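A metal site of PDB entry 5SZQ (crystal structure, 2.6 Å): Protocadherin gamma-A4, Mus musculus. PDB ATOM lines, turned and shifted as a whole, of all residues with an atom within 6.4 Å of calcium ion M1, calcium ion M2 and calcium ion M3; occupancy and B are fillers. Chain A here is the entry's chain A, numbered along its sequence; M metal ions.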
ATOM      1  N   GLU A 226     -33.762  35.250 -11.238  1.00  0.00           N
ATOM      2  CA  GLU A 226     -34.183  35.186  -9.837  1.00  0.00           C
ATOM      3  C   GLU A 226     -34.032  36.536  -9.151  1.00  0.00           C
ATOM      4  O   GLU A 226     -35.026  37.193  -8.834  1.00  0.00           O
ATOM      5  CB  GLU A 226     -33.387  34.134  -9.077  1.00  0.00           C
ATOM      6  CG  GLU A 226     -33.748  34.065  -7.605  1.00  0.00           C
ATOM      7  CD  GLU A 226     -33.075  32.921  -6.906  1.00  0.00           C
ATOM      8  OE1 GLU A 226     -32.384  32.150  -7.600  1.00  0.00           O
ATOM      9  OE2 GLU A 226     -33.225  32.800  -5.670  1.00  0.00           O
ATOM     10  N   ASN A 227     -32.799  36.966  -8.899  1.00  0.00           N
ATOM     11  CA  ASN A 227     -32.580  38.310  -8.411  1.00  0.00           C
ATOM     12  C   ASN A 227     -32.635  39.258  -9.592  1.00  0.00           C
ATOM     13  O   ASN A 227     -32.140  38.940 -10.680  1.00  0.00           O
ATOM     14  CB  ASN A 227     -31.228  38.411  -7.687  1.00  0.00           C
ATOM     15  CG  ASN A 227     -31.015  37.309  -6.640  1.00  0.00           C
ATOM     16  OD1 ASN A 227     -31.846  36.408  -6.481  1.00  0.00           O
ATOM     17  ND2 ASN A 227     -29.882  37.362  -5.950  1.00  0.00           N
ATOM     18  N   ASP A 284     -37.512  36.277  -5.724  1.00  0.00           N
ATOM     19  CA  ASP A 284     -36.722  35.144  -5.247  1.00  0.00           C
ATOM     20  C   ASP A 284     -37.366  33.845  -5.726  1.00  0.00           C
ATOM     21  O   ASP A 284     -38.528  33.573  -5.412  1.00  0.00           O
ATOM     22  CB  ASP A 284     -36.619  35.160  -3.726  1.00  0.00           C
ATOM     23  CG  ASP A 284     -35.759  34.042  -3.200  1.00  0.00           C
ATOM     24  OD1 ASP A 284     -34.897  33.548  -3.950  1.00  0.00           O
ATOM     25  OD2 ASP A 284     -35.958  33.625  -2.038  1.00  0.00           O
ATOM     26  N   TYR A 285     -36.600  33.044  -6.469  1.00  0.00           N
ATOM     27  CA  TYR A 285     -37.176  31.837  -7.075  1.00  0.00           C
ATOM     28  C   TYR A 285     -37.642  30.851  -6.017  1.00  0.00           C
ATOM     29  O   TYR A 285     -38.624  30.133  -6.229  1.00  0.00           O
ATOM     30  CB  TYR A 285     -36.169  31.164  -7.997  1.00  0.00           C
ATOM     31  CG  TYR A 285     -36.734  29.954  -8.730  1.00  0.00           C
ATOM     32  CD1 TYR A 285     -37.380  30.093  -9.940  1.00  0.00           C
ATOM     33  CD2 TYR A 285     -36.635  28.679  -8.190  1.00  0.00           C
ATOM     34  CE1 TYR A 285     -37.902  29.006 -10.608  1.00  0.00           C
ATOM     35  CE2 TYR A 285     -37.163  27.571  -8.861  1.00  0.00           C
ATOM     36  CZ  TYR A 285     -37.790  27.751 -10.073  1.00  0.00           C
ATOM     37  OH  TYR A 285     -38.316  26.671 -10.746  1.00  0.00           O
ATOM     38  N   GLU A 286     -36.966  30.797  -4.872  1.00  0.00           N
ATOM     39  CA  GLU A 286     -37.354  29.885  -3.806  1.00  0.00           C
ATOM     40  C   GLU A 286     -38.569  30.364  -3.039  1.00  0.00           C
ATOM     41  O   GLU A 286     -39.084  29.611  -2.194  1.00  0.00           O
ATOM     42  CB  GLU A 286     -36.187  29.660  -2.854  1.00  0.00           C
ATOM     43  CG  GLU A 286     -35.055  28.844  -3.461  1.00  0.00           C
ATOM     44  CD  GLU A 286     -34.256  29.629  -4.498  1.00  0.00           C
ATOM     45  OE1 GLU A 286     -34.036  30.837  -4.278  1.00  0.00           O
ATOM     46  OE2 GLU A 286     -33.863  29.031  -5.520  1.00  0.00           O
ATOM     47  N   LEU A 316     -36.821  32.551 -13.363  1.00  0.00           N
ATOM     48  CA  LEU A 316     -35.787  31.562 -13.640  1.00  0.00           C
ATOM     49  C   LEU A 316     -34.913  31.384 -12.404  1.00  0.00           C
ATOM     50  O   LEU A 316     -34.480  32.371 -11.805  1.00  0.00           O
ATOM     51  CB  LEU A 316     -34.941  31.975 -14.844  1.00  0.00           C
ATOM     52  CG  LEU A 316     -35.662  32.114 -16.192  1.00  0.00           C
ATOM     53  CD1 LEU A 316     -34.735  32.685 -17.247  1.00  0.00           C
ATOM     54  CD2 LEU A 316     -36.223  30.777 -16.644  1.00  0.00           C
ATOM     55  N   ASP A 317     -34.673  30.130 -12.038  1.00  0.00           N
ATOM     56  CA  ASP A 317     -33.867  29.816 -10.861  1.00  0.00           C
ATOM     57  C   ASP A 317     -32.415  30.223 -11.074  1.00  0.00           C
ATOM     58  O   ASP A 317     -31.877  30.136 -12.182  1.00  0.00           O
ATOM     59  CB  ASP A 317     -33.944  28.325 -10.552  1.00  0.00           C
ATOM     60  CG  ASP A 317     -33.097  27.940  -9.355  1.00  0.00           C
ATOM     61  OD1 ASP A 317     -33.174  28.629  -8.312  1.00  0.00           O
ATOM     62  OD2 ASP A 317     -32.337  26.965  -9.463  1.00  0.00           O
ATOM     63  N   GLN A 318     -31.783  30.678  -9.999  1.00  0.00           N
ATOM     64  CA  GLN A 318     -30.378  31.055 -10.005  1.00  0.00           C
ATOM     65  C   GLN A 318     -29.660  30.367  -8.859  1.00  0.00           C
ATOM     66  O   GLN A 318     -30.211  30.234  -7.762  1.00  0.00           O
ATOM     67  CB  GLN A 318     -30.216  32.583  -9.897  1.00  0.00           C
ATOM     68  CG  GLN A 318     -28.787  33.040  -9.713  1.00  0.00           C
ATOM     69  CD  GLN A 318     -28.618  34.530  -9.881  1.00  0.00           C
ATOM     70  OE1 GLN A 318     -29.077  35.118 -10.868  1.00  0.00           O
ATOM     71  NE2 GLN A 318     -27.952  35.165  -8.921  1.00  0.00           N
ATOM     72  N   ASN A 319     -28.430  29.915  -9.122  1.00  0.00           N
ATOM     73  CA  ASN A 319     -27.587  29.287  -8.102  1.00  0.00           C
ATOM     74  C   ASN A 319     -27.099  30.372  -7.149  1.00  0.00           C
ATOM     75  O   ASN A 319     -26.001  30.925  -7.286  1.00  0.00           O
ATOM     76  CB  ASN A 319     -26.427  28.517  -8.730  1.00  0.00           C
ATOM     77  CG  ASN A 319     -25.632  27.729  -7.705  1.00  0.00           C
ATOM     78  OD1 ASN A 319     -26.090  27.514  -6.592  1.00  0.00           O
ATOM     79  ND2 ASN A 319     -24.444  27.297  -8.091  1.00  0.00           N
ATOM     80  N   ASP A 320     -27.952  30.699  -6.175  1.00  0.00           N
ATOM     81  CA  ASP A 320     -27.658  31.727  -5.176  1.00  0.00           C
ATOM     82  C   ASP A 320     -27.810  31.180  -3.761  1.00  0.00           C
ATOM     83  O   ASP A 320     -28.103  31.936  -2.831  1.00  0.00           O
ATOM     84  CB  ASP A 320     -28.558  32.939  -5.381  1.00  0.00           C
ATOM     85  CG  ASP A 320     -30.005  32.674  -4.990  1.00  0.00           C
ATOM     86  OD1 ASP A 320     -30.481  31.531  -5.196  1.00  0.00           O
ATOM     87  OD2 ASP A 320     -30.657  33.612  -4.488  1.00  0.00           O
ATOM     88  N   ASN A 321     -27.612  29.870  -3.577  1.00  0.00           N
ATOM     89  CA  ASN A 321     -27.723  29.233  -2.276  1.00  0.00           C
ATOM     90  C   ASN A 321     -26.649  28.169  -2.148  1.00  0.00           C
ATOM     91  O   ASN A 321     -26.575  27.248  -2.984  1.00  0.00           O
ATOM     92  CB  ASN A 321     -29.108  28.608  -2.067  1.00  0.00           C
ATOM     93  CG  ASN A 321     -30.142  29.624  -1.643  1.00  0.00           C
ATOM     94  OD1 ASN A 321     -29.893  30.452  -0.768  1.00  0.00           O
ATOM     95  ND2 ASN A 321     -31.318  29.571  -2.277  1.00  0.00           N
ATOM     96  N   THR A 322     -25.821  28.289  -1.120  1.00  0.00           N
ATOM     97  CA  THR A 322     -24.839  27.265  -0.822  1.00  0.00           C
ATOM     98  C   THR A 322     -25.549  26.021  -0.284  1.00  0.00           C
ATOM     99  O   THR A 322     -26.610  26.125   0.348  1.00  0.00           O
ATOM    100  CB  THR A 322     -23.839  27.775   0.219  1.00  0.00           C
ATOM    101  OG1 THR A 322     -23.369  29.074  -0.165  1.00  0.00           O
ATOM    102  CG2 THR A 322     -22.642  26.839   0.347  1.00  0.00           C
ATOM    103  N   PRO A 323     -25.031  24.832  -0.562  1.00  0.00           N
ATOM    104  CA  PRO A 323     -25.572  23.622   0.073  1.00  0.00           C
ATOM    105  C   PRO A 323     -25.438  23.672   1.592  1.00  0.00           C
ATOM    106  O   PRO A 323     -24.463  24.190   2.128  1.00  0.00           O
ATOM    107  CB  PRO A 323     -24.727  22.500  -0.539  1.00  0.00           C
ATOM    108  CG  PRO A 323     -24.302  23.033  -1.863  1.00  0.00           C
ATOM    109  CD  PRO A 323     -24.129  24.510  -1.682  1.00  0.00           C
ATOM    110  N   ASP A 358     -30.025  21.532  -0.699  1.00  0.00           N
ATOM    111  CA  ASP A 358     -29.747  22.779  -1.405  1.00  0.00           C
ATOM    112  C   ASP A 358     -31.075  23.447  -1.758  1.00  0.00           C
ATOM    113  O   ASP A 358     -31.923  22.827  -2.408  1.00  0.00           O
ATOM    114  CB  ASP A 358     -28.915  22.527  -2.670  1.00  0.00           C
ATOM    115  CG  ASP A 358     -28.396  23.804  -3.293  1.00  0.00           C
ATOM    116  OD1 ASP A 358     -27.164  23.920  -3.480  1.00  0.00           O
ATOM    117  OD2 ASP A 358     -29.206  24.695  -3.618  1.00  0.00           O
ATOM    118  N   LYS A 359     -31.255  24.702  -1.326  1.00  0.00           N
ATOM    119  CA  LYS A 359     -32.537  25.382  -1.500  1.00  0.00           C
ATOM    120  C   LYS A 359     -32.900  25.569  -2.975  1.00  0.00           C
ATOM    121  O   LYS A 359     -34.087  25.692  -3.300  1.00  0.00           O
ATOM    122  CB  LYS A 359     -32.533  26.742  -0.801  1.00  0.00           C
ATOM    123  CG  LYS A 359     -32.548  26.678   0.704  1.00  0.00           C
ATOM    124  CD  LYS A 359     -32.507  28.063   1.310  1.00  0.00           C
ATOM    125  CE  LYS A 359     -32.448  27.989   2.829  1.00  0.00           C
ATOM    126  NZ  LYS A 359     -32.294  29.334   3.450  1.00  0.00           N
ATOM    127  N   ASP A 360     -31.910  25.611  -3.857  1.00  0.00           N
ATOM    128  CA  ASP A 360     -32.126  25.872  -5.274  1.00  0.00           C
ATOM    129  C   ASP A 360     -32.795  24.653  -5.925  1.00  0.00           C
ATOM    130  O   ASP A 360     -33.247  23.718  -5.257  1.00  0.00           O
ATOM    131  CB  ASP A 360     -30.811  26.227  -5.952  1.00  0.00           C
ATOM    132  CG  ASP A 360     -30.058  27.334  -5.222  1.00  0.00           C
ATOM    133  OD1 ASP A 360     -30.656  28.403  -4.990  1.00  0.00           O
ATOM    134  OD2 ASP A 360     -28.879  27.130  -4.866  1.00  0.00           O
ATOM    135  N   SER A 361     -32.859  24.650  -7.260  1.00  0.00           N
ATOM    136  CA  SER A 361     -33.527  23.593  -8.000  1.00  0.00           C
ATOM    137  C   SER A 361     -32.632  23.142  -9.151  1.00  0.00           C
ATOM    138  O   SER A 361     -31.613  23.771  -9.454  1.00  0.00           O
ATOM    139  CB  SER A 361     -34.893  24.071  -8.526  1.00  0.00           C
ATOM    140  OG  SER A 361     -35.633  23.006  -9.084  1.00  0.00           O
ATOM    141  N   GLN A 363     -30.008  21.662 -11.671  1.00  0.00           N
ATOM    142  CA  GLN A 363     -28.568  21.483 -11.514  1.00  0.00           C
ATOM    143  C   GLN A 363     -28.032  22.251 -10.322  1.00  0.00           C
ATOM    144  O   GLN A 363     -27.013  21.861  -9.747  1.00  0.00           O
ATOM    145  CB  GLN A 363     -27.824  21.912 -12.774  1.00  0.00           C
ATOM    146  CG  GLN A 363     -27.910  20.918 -13.914  1.00  0.00           C
ATOM    147  CD  GLN A 363     -26.882  21.189 -14.998  1.00  0.00           C
ATOM    148  OE1 GLN A 363     -26.164  22.178 -14.944  1.00  0.00           O
ATOM    149  NE2 GLN A 363     -26.813  20.312 -15.996  1.00  0.00           N
ATOM    150  N   ASN A 364     -28.692  23.352  -9.919  1.00  0.00           N
ATOM    151  CA  ASN A 364     -28.242  24.087  -8.749  1.00  0.00           C
ATOM    152  C   ASN A 364     -28.539  23.354  -7.443  1.00  0.00           C
ATOM    153  O   ASN A 364     -28.001  23.741  -6.390  1.00  0.00           O
ATOM    154  CB  ASN A 364     -28.882  25.479  -8.750  1.00  0.00           C
ATOM    155  CG  ASN A 364     -28.756  26.198 -10.090  1.00  0.00           C
ATOM    156  OD1 ASN A 364     -27.962  25.819 -10.947  1.00  0.00           O
ATOM    157  ND2 ASN A 364     -29.549  27.256 -10.271  1.00  0.00           N
ATOM    158  N   ALA A 365     -29.390  22.317  -7.477  1.00  0.00           N
ATOM    159  CA  ALA A 365     -29.660  21.478  -6.311  1.00  0.00           C
ATOM    160  C   ALA A 365     -29.065  20.083  -6.460  1.00  0.00           C
ATOM    161  O   ALA A 365     -29.439  19.179  -5.711  1.00  0.00           O
ATOM    162  CB  ALA A 365     -31.162  21.382  -6.062  1.00  0.00           C
ATOM    163  N   LEU A 367     -26.156  17.732  -5.906  1.00  0.00           N
ATOM    164  CA  LEU A 367     -25.022  17.684  -4.995  1.00  0.00           C
ATOM    165  C   LEU A 367     -24.081  16.537  -5.336  1.00  0.00           C
ATOM    166  O   LEU A 367     -24.517  15.437  -5.689  1.00  0.00           O
ATOM    167  CB  LEU A 367     -25.494  17.533  -3.546  1.00  0.00           C
ATOM    168  CG  LEU A 367     -26.145  18.759  -2.918  1.00  0.00           C
ATOM    169  CD1 LEU A 367     -25.514  20.029  -3.464  1.00  0.00           C
ATOM    170  CD2 LEU A 367     -27.642  18.758  -3.144  1.00  0.00           C
ATOM    171  N   ASP A 411     -22.654  21.951  -5.359  1.00  0.00           N
ATOM    172  CA  ASP A 411     -23.763  21.968  -6.297  1.00  0.00           C
ATOM    173  C   ASP A 411     -23.216  22.045  -7.720  1.00  0.00           C
ATOM    174  O   ASP A 411     -22.071  22.447  -7.945  1.00  0.00           O
ATOM    175  CB  ASP A 411     -24.709  23.132  -6.003  1.00  0.00           C
ATOM    176  CG  ASP A 411     -24.027  24.484  -6.045  1.00  0.00           C
ATOM    177  OD1 ASP A 411     -22.779  24.527  -6.154  1.00  0.00           O
ATOM    178  OD2 ASP A 411     -24.734  25.503  -5.964  1.00  0.00           O
ATOM    179  N   HIS A 412     -24.042  21.632  -8.680  1.00  0.00           N
ATOM    180  CA  HIS A 412     -23.616  21.562 -10.073  1.00  0.00           C
ATOM    181  C   HIS A 412     -24.117  22.749 -10.906  1.00  0.00           C
ATOM    182  O   HIS A 412     -24.260  22.625 -12.121  1.00  0.00           O
ATOM    183  CB  HIS A 412     -24.071  20.248 -10.703  1.00  0.00           C
ATOM    184  CG  HIS A 412     -23.234  19.072 -10.286  1.00  0.00           C
ATOM    185  ND1 HIS A 412     -23.785  17.915  -9.777  1.00  0.00           N
ATOM    186  CD2 HIS A 412     -21.898  18.883 -10.307  1.00  0.00           C
ATOM    187  CE1 HIS A 412     -22.816  17.054  -9.500  1.00  0.00           C
ATOM    188  NE2 HIS A 412     -21.663  17.618  -9.821  1.00  0.00           N
ATOM    189  N   GLY A 413     -24.383  23.877 -10.263  1.00  0.00           N
ATOM    190  CA  GLY A 413     -24.807  25.069 -10.970  1.00  0.00           C
ATOM    191  C   GLY A 413     -23.628  25.885 -11.493  1.00  0.00           C
ATOM    192  O   GLY A 413     -22.464  25.489 -11.385  1.00  0.00           O
ATOM    193  N   LEU A 417     -21.071  26.184  -5.886  1.00  0.00           N
ATOM    194  CA  LEU A 417     -20.828  26.564  -4.503  1.00  0.00           C
ATOM    195  C   LEU A 417     -20.559  25.328  -3.660  1.00  0.00           C
ATOM    196  O   LEU A 417     -21.170  24.269  -3.879  1.00  0.00           O
ATOM    197  CB  LEU A 417     -22.022  27.347  -3.922  1.00  0.00           C
ATOM    198  CG  LEU A 417     -22.574  28.491  -4.782  1.00  0.00           C
ATOM    199  CD1 LEU A 417     -23.884  29.039  -4.195  1.00  0.00           C
ATOM    200  CD2 LEU A 417     -21.551  29.614  -4.957  1.00  0.00           C
HETATM  201 CA    CA M   1     -26.943  25.835  -5.058  1.00  0.00          CA
HETATM  202 CA    CA M   2     -32.216  30.074  -6.408  1.00  0.00          CA
HETATM  203 CA    CA M   3     -32.622  33.687  -3.609  1.00  0.00          CA
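The side-chain amide nitrogen (ND2) of Asn 364 sits at hydrogen-bond distance from the side-chain carboxylate (OD2) of Asp 317, at 2.9 Å.
The side-chain carboxylate (OD2) of Asp 317 is in hydrogen-bond range of the backbone NH (N) of Ser 361 (3.2 Å).
The backbone NH (N) of Asp 411 sits at hydrogen-bond distance from the backbone carbonyl oxygen (O) of Leu 417 (3.1 Å).
N of Glu 226 sits at hydrogen-bond distance from O of Leu 316 (3.0 Å).
OE2 of Glu 226 lies close to N of Tyr 285 (3.5 Å).
Of the 25 residues printed, 6 come within 4 Å of calcium ion M1.
The nearest printed residue that does not touch calcium ion M1 is Leu 417 (4.5 Å).
Of the 25 residues printed, 6 come within 4 Å of calcium ion M2.
Along chain A the residues within 4 Å of calcium ion M2 span positions 226 to 360.
Of the 25 residues printed, 4 come within 4 Å of calcium ion M3.
Calcium ion M1 is bound by the side-chain carboxylate (OD2) of Asp 360, the side-chain carboxylate (OD2) of Asp 411, the side-chain amide oxygen (OD1) of Asn 319, the side-chain carboxylate (OD1) of Asp 358, the backbone carbonyl oxygen (O) of Asn 321 and the backbone carbonyl oxygen (O) of Asn 364.
Slightly farther from calcium ion M1 lies the side-chain carboxylate (OD2) of Asp 358 (2.9 Å).
Calcium ion M2 is bound by OE2 of Glu 286 (2.1 Å), OE1 of Glu 226 (2.4 Å), O of Gln 318 (2.4 Å), OD1 of Asp 320 (2.6 Å), OD1 of Asp 317 (2.6 Å) and OD1 of Asp 360 (2.7 Å).
Calcium ion M2 has six donor atoms within binding distance.
Slightly farther from calcium ion M2 lies OE1 of Glu 286 (2.9 Å).
Slightly farther from calcium ion M2 lies the side-chain carboxylate (OE2) of Glu 226 (3.0 Å).
Calcium ion M3 is bound by OD2 of Asp 320 (2.2 Å), OD1 of Asp 284 (2.3 Å) and OE2 of Glu 226 (2.3 Å).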
